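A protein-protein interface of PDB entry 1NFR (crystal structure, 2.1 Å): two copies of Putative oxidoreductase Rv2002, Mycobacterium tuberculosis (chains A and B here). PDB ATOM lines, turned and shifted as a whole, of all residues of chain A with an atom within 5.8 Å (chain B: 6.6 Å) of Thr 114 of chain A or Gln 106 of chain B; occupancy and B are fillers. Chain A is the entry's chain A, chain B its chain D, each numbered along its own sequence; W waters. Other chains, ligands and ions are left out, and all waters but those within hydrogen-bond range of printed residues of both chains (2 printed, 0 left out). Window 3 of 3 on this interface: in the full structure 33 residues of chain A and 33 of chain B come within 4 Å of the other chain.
OG1 of Thr 114 of chain A is in hydrogen-bond range of NE1 of Trp 105 of chain B (3.0 Å). The side-chain hydroxyl (OG1) of Thr 114 of chain A lies within hydrogen-bond range of the side-chain amide nitrogen (NE2) of Gln 106 of chain B.
Water W1 lies within hydrogen-bond range of OD1 of Asp 110 of chain A (2.5 Å), NE2 of Gln 106 of chain B (2.5 Å) and OG1 of Thr 114 of chain A (2.6 Å). Water W2 bridges OD1 of Asp 110 of chain B (2.5 Å) and NE2 of Gln 106 of chain A (2.8 Å).
Hydrophobic or aromatic side chains of chain B that line the printed part of chain A: Tyr 100, Leu 102, Trp 105 and Leu 109. Hydrophobic or aromatic side chains of chain A within 4 Å of the printed part of chain B: Leu 113, Phe 117 and Leu 118. Among the printed residues, no Asp or Glu carboxylate lies within 4 Å of a Lys or Arg side-chain nitrogen of the other chain.
Among the printed residues, pairs that only touch across the chains: Leu 113 of chain A with Trp 105 of chain B (3.8 Å), Thr 114 of chain A with Leu 109 of chain B (3.7 Å), Phe 117 of chain A with Tyr 100 of chain B (3.7 Å), Phe 117 of chain A with Trp 105 of chain B (3.6 Å) and Leu 118 of chain A with Leu 102 of chain B (3.8 Å).
5 positions are printed for both chains. Of the 7 pairs that touch across the chains among the printed residues, none has its exchanged pair printed and touching as well.
N of Thr 114 of chain A is in hydrogen-bond range of O of Leu 109 of chain A (2.8 Å). The backbone carbonyl oxygen (O) of Gln 106 of chain B lies close to the side-chain carboxylate (OD2) of Asp 110 of chain B (2.7 Å).
Printed residues of chain B within 4 Å of Leu 113 of chain A: Trp 105 (3.8 Å). Thr 114 of chain A touches just these residues of chain B: Trp 105, Gln 106 and Leu 109. Printed residues of chain B within 4 Å of Leu 118 of chain A: Leu 102 (3.8 Å). Printed residues of chain A within 4 Å of Trp 105 of chain B: Leu 113, Thr 114 and Phe 117. Gln 106 of chain B touches one residue of chain A. Val 111 of chain B touches none of the printed residues of chain A. The nearest printed residue of chain B that does not touch Leu 118 of chain A is Trp 105 of chain B (6.4 Å).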
ATOM      1  N   VAL A  62      28.313  12.307  16.494  1.00  0.00           N
ATOM      2  CA  VAL A  62      28.243  10.865  16.338  1.00  0.00           C
ATOM      3  C   VAL A  62      28.292  10.353  14.905  1.00  0.00           C
ATOM      4  O   VAL A  62      28.492   9.161  14.687  1.00  0.00           O
ATOM      5  CB  VAL A  62      26.998  10.286  17.040  1.00  0.00           C
ATOM      6  CG1 VAL A  62      27.080  10.568  18.536  1.00  0.00           C
ATOM      7  CG2 VAL A  62      25.738  10.884  16.450  1.00  0.00           C
ATOM      8  N   THR A  63      28.122  11.241  13.928  1.00  0.00           N
ATOM      9  CA  THR A  63      28.161  10.811  12.532  1.00  0.00           C
ATOM     10  C   THR A  63      29.595  10.780  12.015  1.00  0.00           C
ATOM     11  O   THR A  63      29.849  10.329  10.895  1.00  0.00           O
ATOM     12  CB  THR A  63      27.308  11.732  11.618  1.00  0.00           C
ATOM     13  OG1 THR A  63      27.824  13.069  11.650  1.00  0.00           O
ATOM     14  CG2 THR A  63      25.848  11.734  12.078  1.00  0.00           C
ATOM     15  N   GLN A 106      17.388  11.026   5.579  1.00  0.00           N
ATOM     16  CA  GLN A 106      18.799  10.668   5.560  1.00  0.00           C
ATOM     17  C   GLN A 106      19.456  11.124   6.849  1.00  0.00           C
ATOM     18  O   GLN A 106      20.172  10.365   7.489  1.00  0.00           O
ATOM     19  CB  GLN A 106      19.508  11.307   4.365  1.00  0.00           C
ATOM     20  CG  GLN A 106      19.306  10.554   3.054  1.00  0.00           C
ATOM     21  CD  GLN A 106      19.513   9.055   3.217  1.00  0.00           C
ATOM     22  OE1 GLN A 106      20.414   8.620   3.928  1.00  0.00           O
ATOM     23  NE2 GLN A 106      18.681   8.261   2.551  1.00  0.00           N
ATOM     24  N   ILE A 108      18.218  11.711   9.915  1.00  0.00           N
ATOM     25  CA  ILE A 108      17.888  10.943  11.112  1.00  0.00           C
ATOM     26  C   ILE A 108      18.506   9.544  11.101  1.00  0.00           C
ATOM     27  O   ILE A 108      18.843   9.006  12.156  1.00  0.00           O
ATOM     28  CB  ILE A 108      16.361  10.850  11.326  1.00  0.00           C
ATOM     29  CG1 ILE A 108      16.085  10.309  12.731  1.00  0.00           C
ATOM     30  CG2 ILE A 108      15.723   9.974  10.252  1.00  0.00           C
ATOM     31  CD1 ILE A 108      14.664  10.493  13.199  1.00  0.00           C
ATOM     32  N   LEU A 109      18.668   8.954   9.918  1.00  0.00           N
ATOM     33  CA  LEU A 109      19.299   7.640   9.831  1.00  0.00           C
ATOM     34  C   LEU A 109      20.768   7.809  10.212  1.00  0.00           C
ATOM     35  O   LEU A 109      21.344   6.966  10.913  1.00  0.00           O
ATOM     36  CB  LEU A 109      19.208   7.069   8.410  1.00  0.00           C
ATOM     37  CG  LEU A 109      18.040   6.139   8.053  1.00  0.00           C
ATOM     38  CD1 LEU A 109      16.720   6.866   8.230  1.00  0.00           C
ATOM     39  CD2 LEU A 109      18.197   5.654   6.621  1.00  0.00           C
ATOM     40  N   ASP A 110      21.363   8.914   9.754  1.00  0.00           N
ATOM     41  CA  ASP A 110      22.772   9.214  10.029  1.00  0.00           C
ATOM     42  C   ASP A 110      23.073   9.329  11.523  1.00  0.00           C
ATOM     43  O   ASP A 110      24.003   8.712  12.025  1.00  0.00           O
ATOM     44  CB  ASP A 110      23.201  10.532   9.361  1.00  0.00           C
ATOM     45  CG  ASP A 110      23.298  10.437   7.847  1.00  0.00           C
ATOM     46  OD1 ASP A 110      23.307   9.313   7.295  1.00  0.00           O
ATOM     47  OD2 ASP A 110      23.383  11.504   7.203  1.00  0.00           O
ATOM     48  N   VAL A 111      22.285  10.135  12.224  1.00  0.00           N
ATOM     49  CA  VAL A 111      22.492  10.351  13.653  1.00  0.00           C
ATOM     50  C   VAL A 111      21.964   9.231  14.548  1.00  0.00           C
ATOM     51  O   VAL A 111      22.717   8.644  15.328  1.00  0.00           O
ATOM     52  CB  VAL A 111      21.830  11.673  14.118  1.00  0.00           C
ATOM     53  CG1 VAL A 111      22.094  11.894  15.597  1.00  0.00           C
ATOM     54  CG2 VAL A 111      22.354  12.851  13.298  1.00  0.00           C
ATOM     55  N   ASN A 112      20.667   8.957  14.420  1.00  0.00           N
ATOM     56  CA  ASN A 112      19.973   7.956  15.221  1.00  0.00           C
ATOM     57  C   ASN A 112      20.368   6.505  14.987  1.00  0.00           C
ATOM     58  O   ASN A 112      20.331   5.701  15.918  1.00  0.00           O
ATOM     59  CB  ASN A 112      18.457   8.095  15.020  1.00  0.00           C
ATOM     60  CG  ASN A 112      17.875   9.287  15.751  1.00  0.00           C
ATOM     61  OD1 ASN A 112      18.586  10.225  16.107  1.00  0.00           O
ATOM     62  ND2 ASN A 112      16.561   9.262  15.963  1.00  0.00           N
ATOM     63  N   LEU A 113      20.743   6.166  13.759  1.00  0.00           N
ATOM     64  CA  LEU A 113      21.114   4.788  13.440  1.00  0.00           C
ATOM     65  C   LEU A 113      22.606   4.585  13.230  1.00  0.00           C
ATOM     66  O   LEU A 113      23.270   3.911  14.014  1.00  0.00           O
ATOM     67  CB  LEU A 113      20.363   4.318  12.185  1.00  0.00           C
ATOM     68  CG  LEU A 113      20.599   2.884  11.708  1.00  0.00           C
ATOM     69  CD1 LEU A 113      20.547   1.916  12.879  1.00  0.00           C
ATOM     70  CD2 LEU A 113      19.529   2.521  10.667  1.00  0.00           C
ATOM     71  N   THR A 114      23.126   5.158  12.152  1.00  0.00           N
ATOM     72  CA  THR A 114      24.539   5.035  11.842  1.00  0.00           C
ATOM     73  C   THR A 114      25.390   5.500  13.020  1.00  0.00           C
ATOM     74  O   THR A 114      26.409   4.881  13.344  1.00  0.00           O
ATOM     75  CB  THR A 114      24.883   5.854  10.583  1.00  0.00           C
ATOM     76  OG1 THR A 114      24.133   5.339   9.473  1.00  0.00           O
ATOM     77  CG2 THR A 114      26.376   5.766  10.270  1.00  0.00           C
ATOM     78  N   GLY A 115      24.958   6.581  13.666  1.00  0.00           N
ATOM     79  CA  GLY A 115      25.693   7.114  14.803  1.00  0.00           C
ATOM     80  C   GLY A 115      25.861   6.111  15.930  1.00  0.00           C
ATOM     81  O   GLY A 115      26.899   6.075  16.596  1.00  0.00           O
ATOM     82  N   VAL A 116      24.826   5.297  16.137  1.00  0.00           N
ATOM     83  CA  VAL A 116      24.819   4.271  17.170  1.00  0.00           C
ATOM     84  C   VAL A 116      25.817   3.182  16.829  1.00  0.00           C
ATOM     85  O   VAL A 116      26.579   2.725  17.688  1.00  0.00           O
ATOM     86  CB  VAL A 116      23.415   3.637  17.301  1.00  0.00           C
ATOM     87  CG1 VAL A 116      23.452   2.461  18.258  1.00  0.00           C
ATOM     88  CG2 VAL A 116      22.432   4.677  17.792  1.00  0.00           C
ATOM     89  N   PHE A 117      25.807   2.761  15.568  1.00  0.00           N
ATOM     90  CA  PHE A 117      26.720   1.721  15.112  1.00  0.00           C
ATOM     91  C   PHE A 117      28.164   2.208  15.205  1.00  0.00           C
ATOM     92  O   PHE A 117      29.040   1.470  15.650  1.00  0.00           O
ATOM     93  CB  PHE A 117      26.380   1.316  13.674  1.00  0.00           C
ATOM     94  CG  PHE A 117      27.188   0.160  13.158  1.00  0.00           C
ATOM     95  CD1 PHE A 117      27.282  -1.026  13.884  1.00  0.00           C
ATOM     96  CD2 PHE A 117      27.831   0.245  11.935  1.00  0.00           C
ATOM     97  CE1 PHE A 117      28.000  -2.103  13.396  1.00  0.00           C
ATOM     98  CE2 PHE A 117      28.558  -0.835  11.433  1.00  0.00           C
ATOM     99  CZ  PHE A 117      28.642  -2.008  12.163  1.00  0.00           C
ATOM    100  N   LEU A 118      28.410   3.451  14.796  1.00  0.00           N
ATOM    101  CA  LEU A 118      29.758   4.001  14.862  1.00  0.00           C
ATOM    102  C   LEU A 118      30.282   3.955  16.295  1.00  0.00           C
ATOM    103  O   LEU A 118      31.423   3.564  16.525  1.00  0.00           O
ATOM    104  CB  LEU A 118      29.788   5.445  14.331  1.00  0.00           C
ATOM    105  CG  LEU A 118      29.517   5.607  12.829  1.00  0.00           C
ATOM    106  CD1 LEU A 118      29.726   7.058  12.421  1.00  0.00           C
ATOM    107  CD2 LEU A 118      30.458   4.701  12.034  1.00  0.00           C
ATOM    108  N   GLY A 119      29.445   4.337  17.254  1.00  0.00           N
ATOM    109  CA  GLY A 119      29.862   4.317  18.650  1.00  0.00           C
ATOM    110  C   GLY A 119      30.328   2.943  19.083  1.00  0.00           C
ATOM    111  O   GLY A 119      31.370   2.801  19.734  1.00  0.00           O
ATOM    112  N   TYR B 100      33.350  -5.248   9.112  1.00  0.00           N
ATOM    113  CA  TYR B 100      32.272  -4.672   8.309  1.00  0.00           C
ATOM    114  C   TYR B 100      32.647  -3.285   7.778  1.00  0.00           C
ATOM    115  O   TYR B 100      32.959  -2.381   8.549  1.00  0.00           O
ATOM    116  CB  TYR B 100      31.001  -4.582   9.164  1.00  0.00           C
ATOM    117  CG  TYR B 100      29.709  -4.408   8.391  1.00  0.00           C
ATOM    118  CD1 TYR B 100      29.398  -5.241   7.315  1.00  0.00           C
ATOM    119  CD2 TYR B 100      28.775  -3.440   8.768  1.00  0.00           C
ATOM    120  CE1 TYR B 100      28.188  -5.119   6.636  1.00  0.00           C
ATOM    121  CE2 TYR B 100      27.560  -3.311   8.098  1.00  0.00           C
ATOM    122  CZ  TYR B 100      27.273  -4.154   7.034  1.00  0.00           C
ATOM    123  OH  TYR B 100      26.069  -4.039   6.379  1.00  0.00           O
ATOM    124  N   ALA B 101      32.615  -3.125   6.457  1.00  0.00           N
ATOM    125  CA  ALA B 101      32.946  -1.845   5.838  1.00  0.00           C
ATOM    126  C   ALA B 101      31.806  -0.846   5.990  1.00  0.00           C
ATOM    127  O   ALA B 101      30.635  -1.201   5.844  1.00  0.00           O
ATOM    128  CB  ALA B 101      33.260  -2.043   4.367  1.00  0.00           C
ATOM    129  N   LEU B 102      32.146   0.406   6.277  1.00  0.00           N
ATOM    130  CA  LEU B 102      31.123   1.425   6.430  1.00  0.00           C
ATOM    131  C   LEU B 102      30.355   1.616   5.131  1.00  0.00           C
ATOM    132  O   LEU B 102      29.190   2.017   5.155  1.00  0.00           O
ATOM    133  CB  LEU B 102      31.734   2.752   6.893  1.00  0.00           C
ATOM    134  CG  LEU B 102      32.201   2.715   8.352  1.00  0.00           C
ATOM    135  CD1 LEU B 102      32.678   4.094   8.791  1.00  0.00           C
ATOM    136  CD2 LEU B 102      31.047   2.242   9.239  1.00  0.00           C
ATOM    137  N   THR B 103      31.003   1.325   4.005  1.00  0.00           N
ATOM    138  CA  THR B 103      30.349   1.449   2.709  1.00  0.00           C
ATOM    139  C   THR B 103      29.268   0.376   2.551  1.00  0.00           C
ATOM    140  O   THR B 103      28.247   0.625   1.912  1.00  0.00           O
ATOM    141  CB  THR B 103      31.357   1.348   1.524  1.00  0.00           C
ATOM    142  OG1 THR B 103      32.194   0.194   1.683  1.00  0.00           O
ATOM    143  CG2 THR B 103      32.220   2.590   1.455  1.00  0.00           C
ATOM    144  N   GLU B 104      29.487  -0.806   3.134  1.00  0.00           N
ATOM    145  CA  GLU B 104      28.500  -1.891   3.054  1.00  0.00           C
ATOM    146  C   GLU B 104      27.277  -1.490   3.885  1.00  0.00           C
ATOM    147  O   GLU B 104      26.136  -1.765   3.519  1.00  0.00           O
ATOM    148  CB  GLU B 104      29.061  -3.208   3.617  1.00  0.00           C
ATOM    149  CG  GLU B 104      30.298  -3.780   2.932  1.00  0.00           C
ATOM    150  CD  GLU B 104      30.768  -5.102   3.568  1.00  0.00           C
ATOM    151  OE1 GLU B 104      30.102  -6.152   3.369  1.00  0.00           O
ATOM    152  OE2 GLU B 104      31.799  -5.093   4.280  1.00  0.00           O
ATOM    153  N   TRP B 105      27.540  -0.851   5.021  1.00  0.00           N
ATOM    154  CA  TRP B 105      26.496  -0.392   5.930  1.00  0.00           C
ATOM    155  C   TRP B 105      25.596   0.618   5.224  1.00  0.00           C
ATOM    156  O   TRP B 105      24.371   0.485   5.236  1.00  0.00           O
ATOM    157  CB  TRP B 105      27.142   0.225   7.177  1.00  0.00           C
ATOM    158  CG  TRP B 105      26.196   0.920   8.123  1.00  0.00           C
ATOM    159  CD1 TRP B 105      25.902   2.251   8.153  1.00  0.00           C
ATOM    160  CD2 TRP B 105      25.437   0.317   9.178  1.00  0.00           C
ATOM    161  NE1 TRP B 105      25.010   2.517   9.161  1.00  0.00           N
ATOM    162  CE2 TRP B 105      24.707   1.347   9.808  1.00  0.00           C
ATOM    163  CE3 TRP B 105      25.305  -0.998   9.655  1.00  0.00           C
ATOM    164  CZ2 TRP B 105      23.851   1.108  10.895  1.00  0.00           C
ATOM    165  CZ3 TRP B 105      24.455  -1.237  10.736  1.00  0.00           C
ATOM    166  CH2 TRP B 105      23.738  -0.186  11.344  1.00  0.00           C
ATOM    167  N   GLN B 106      26.202   1.624   4.601  1.00  0.00           N
ATOM    168  CA  GLN B 106      25.434   2.637   3.881  1.00  0.00           C
ATOM    169  C   GLN B 106      24.642   2.032   2.735  1.00  0.00           C
ATOM    170  O   GLN B 106      23.467   2.350   2.538  1.00  0.00           O
ATOM    171  CB  GLN B 106      26.360   3.720   3.315  1.00  0.00           C
ATOM    172  CG  GLN B 106      26.701   4.806   4.304  1.00  0.00           C
ATOM    173  CD  GLN B 106      25.467   5.341   4.997  1.00  0.00           C
ATOM    174  OE1 GLN B 106      24.453   5.634   4.352  1.00  0.00           O
ATOM    175  NE2 GLN B 106      25.540   5.471   6.315  1.00  0.00           N
ATOM    176  N   ARG B 107      25.303   1.162   1.976  1.00  0.00           N
ATOM    177  CA  ARG B 107      24.688   0.511   0.835  1.00  0.00           C
ATOM    178  C   ARG B 107      23.434  -0.270   1.205  1.00  0.00           C
ATOM    179  O   ARG B 107      22.408  -0.150   0.536  1.00  0.00           O
ATOM    180  CB  ARG B 107      25.694  -0.425   0.160  1.00  0.00           C
ATOM    181  CG  ARG B 107      25.144  -1.152  -1.050  1.00  0.00           C
ATOM    182  CD  ARG B 107      24.600  -0.169  -2.066  1.00  0.00           C
ATOM    183  NE  ARG B 107      23.874  -0.825  -3.151  1.00  0.00           N
ATOM    184  CZ  ARG B 107      23.312  -0.175  -4.164  1.00  0.00           C
ATOM    185  NH1 ARG B 107      23.392   1.146  -4.228  1.00  0.00           N
ATOM    186  NH2 ARG B 107      22.671  -0.850  -5.115  1.00  0.00           N
ATOM    187  N   ILE B 108      23.509  -1.070   2.266  1.00  0.00           N
ATOM    188  CA  ILE B 108      22.349  -1.857   2.664  1.00  0.00           C
ATOM    189  C   ILE B 108      21.250  -0.987   3.279  1.00  0.00           C
ATOM    190  O   ILE B 108      20.074  -1.348   3.233  1.00  0.00           O
ATOM    191  CB  ILE B 108      22.746  -3.024   3.615  1.00  0.00           C
ATOM    192  CG1 ILE B 108      21.569  -4.002   3.739  1.00  0.00           C
ATOM    193  CG2 ILE B 108      23.175  -2.493   4.980  1.00  0.00           C
ATOM    194  CD1 ILE B 108      21.944  -5.351   4.320  1.00  0.00           C
ATOM    195  N   LEU B 109      21.623   0.164   3.835  1.00  0.00           N
ATOM    196  CA  LEU B 109      20.630   1.076   4.397  1.00  0.00           C
ATOM    197  C   LEU B 109      19.850   1.693   3.238  1.00  0.00           C
ATOM    198  O   LEU B 109      18.620   1.785   3.271  1.00  0.00           O
ATOM    199  CB  LEU B 109      21.299   2.194   5.206  1.00  0.00           C
ATOM    200  CG  LEU B 109      21.206   2.114   6.738  1.00  0.00           C
ATOM    201  CD1 LEU B 109      21.886   0.849   7.236  1.00  0.00           C
ATOM    202  CD2 LEU B 109      21.851   3.340   7.355  1.00  0.00           C
ATOM    203  N   ASP B 110      20.579   2.110   2.206  1.00  0.00           N
ATOM    204  CA  ASP B 110      19.975   2.726   1.030  1.00  0.00           C
ATOM    205  C   ASP B 110      18.988   1.801   0.323  1.00  0.00           C
ATOM    206  O   ASP B 110      17.855   2.185   0.033  1.00  0.00           O
ATOM    207  CB  ASP B 110      21.052   3.131   0.026  1.00  0.00           C
ATOM    208  CG  ASP B 110      22.094   4.054   0.620  1.00  0.00           C
ATOM    209  OD1 ASP B 110      21.726   4.950   1.410  1.00  0.00           O
ATOM    210  OD2 ASP B 110      23.285   3.891   0.276  1.00  0.00           O
ATOM    211  N   VAL B 111      19.434   0.581   0.040  1.00  0.00           N
ATOM    212  CA  VAL B 111      18.611  -0.391  -0.666  1.00  0.00           C
ATOM    213  C   VAL B 111      17.514  -1.046   0.164  1.00  0.00           C
ATOM    214  O   VAL B 111      16.345  -1.056  -0.237  1.00  0.00           O
ATOM    215  CB  VAL B 111      19.479  -1.516  -1.265  1.00  0.00           C
ATOM    216  CG1 VAL B 111      18.607  -2.471  -2.070  1.00  0.00           C
ATOM    217  CG2 VAL B 111      20.571  -0.921  -2.136  1.00  0.00           C
HETATM  218  O   HOH W   1      23.781   6.903   7.400  1.00  0.00           O
HETATM  219  O   HOH W   2      19.871   5.711   2.840  1.00  0.00           O
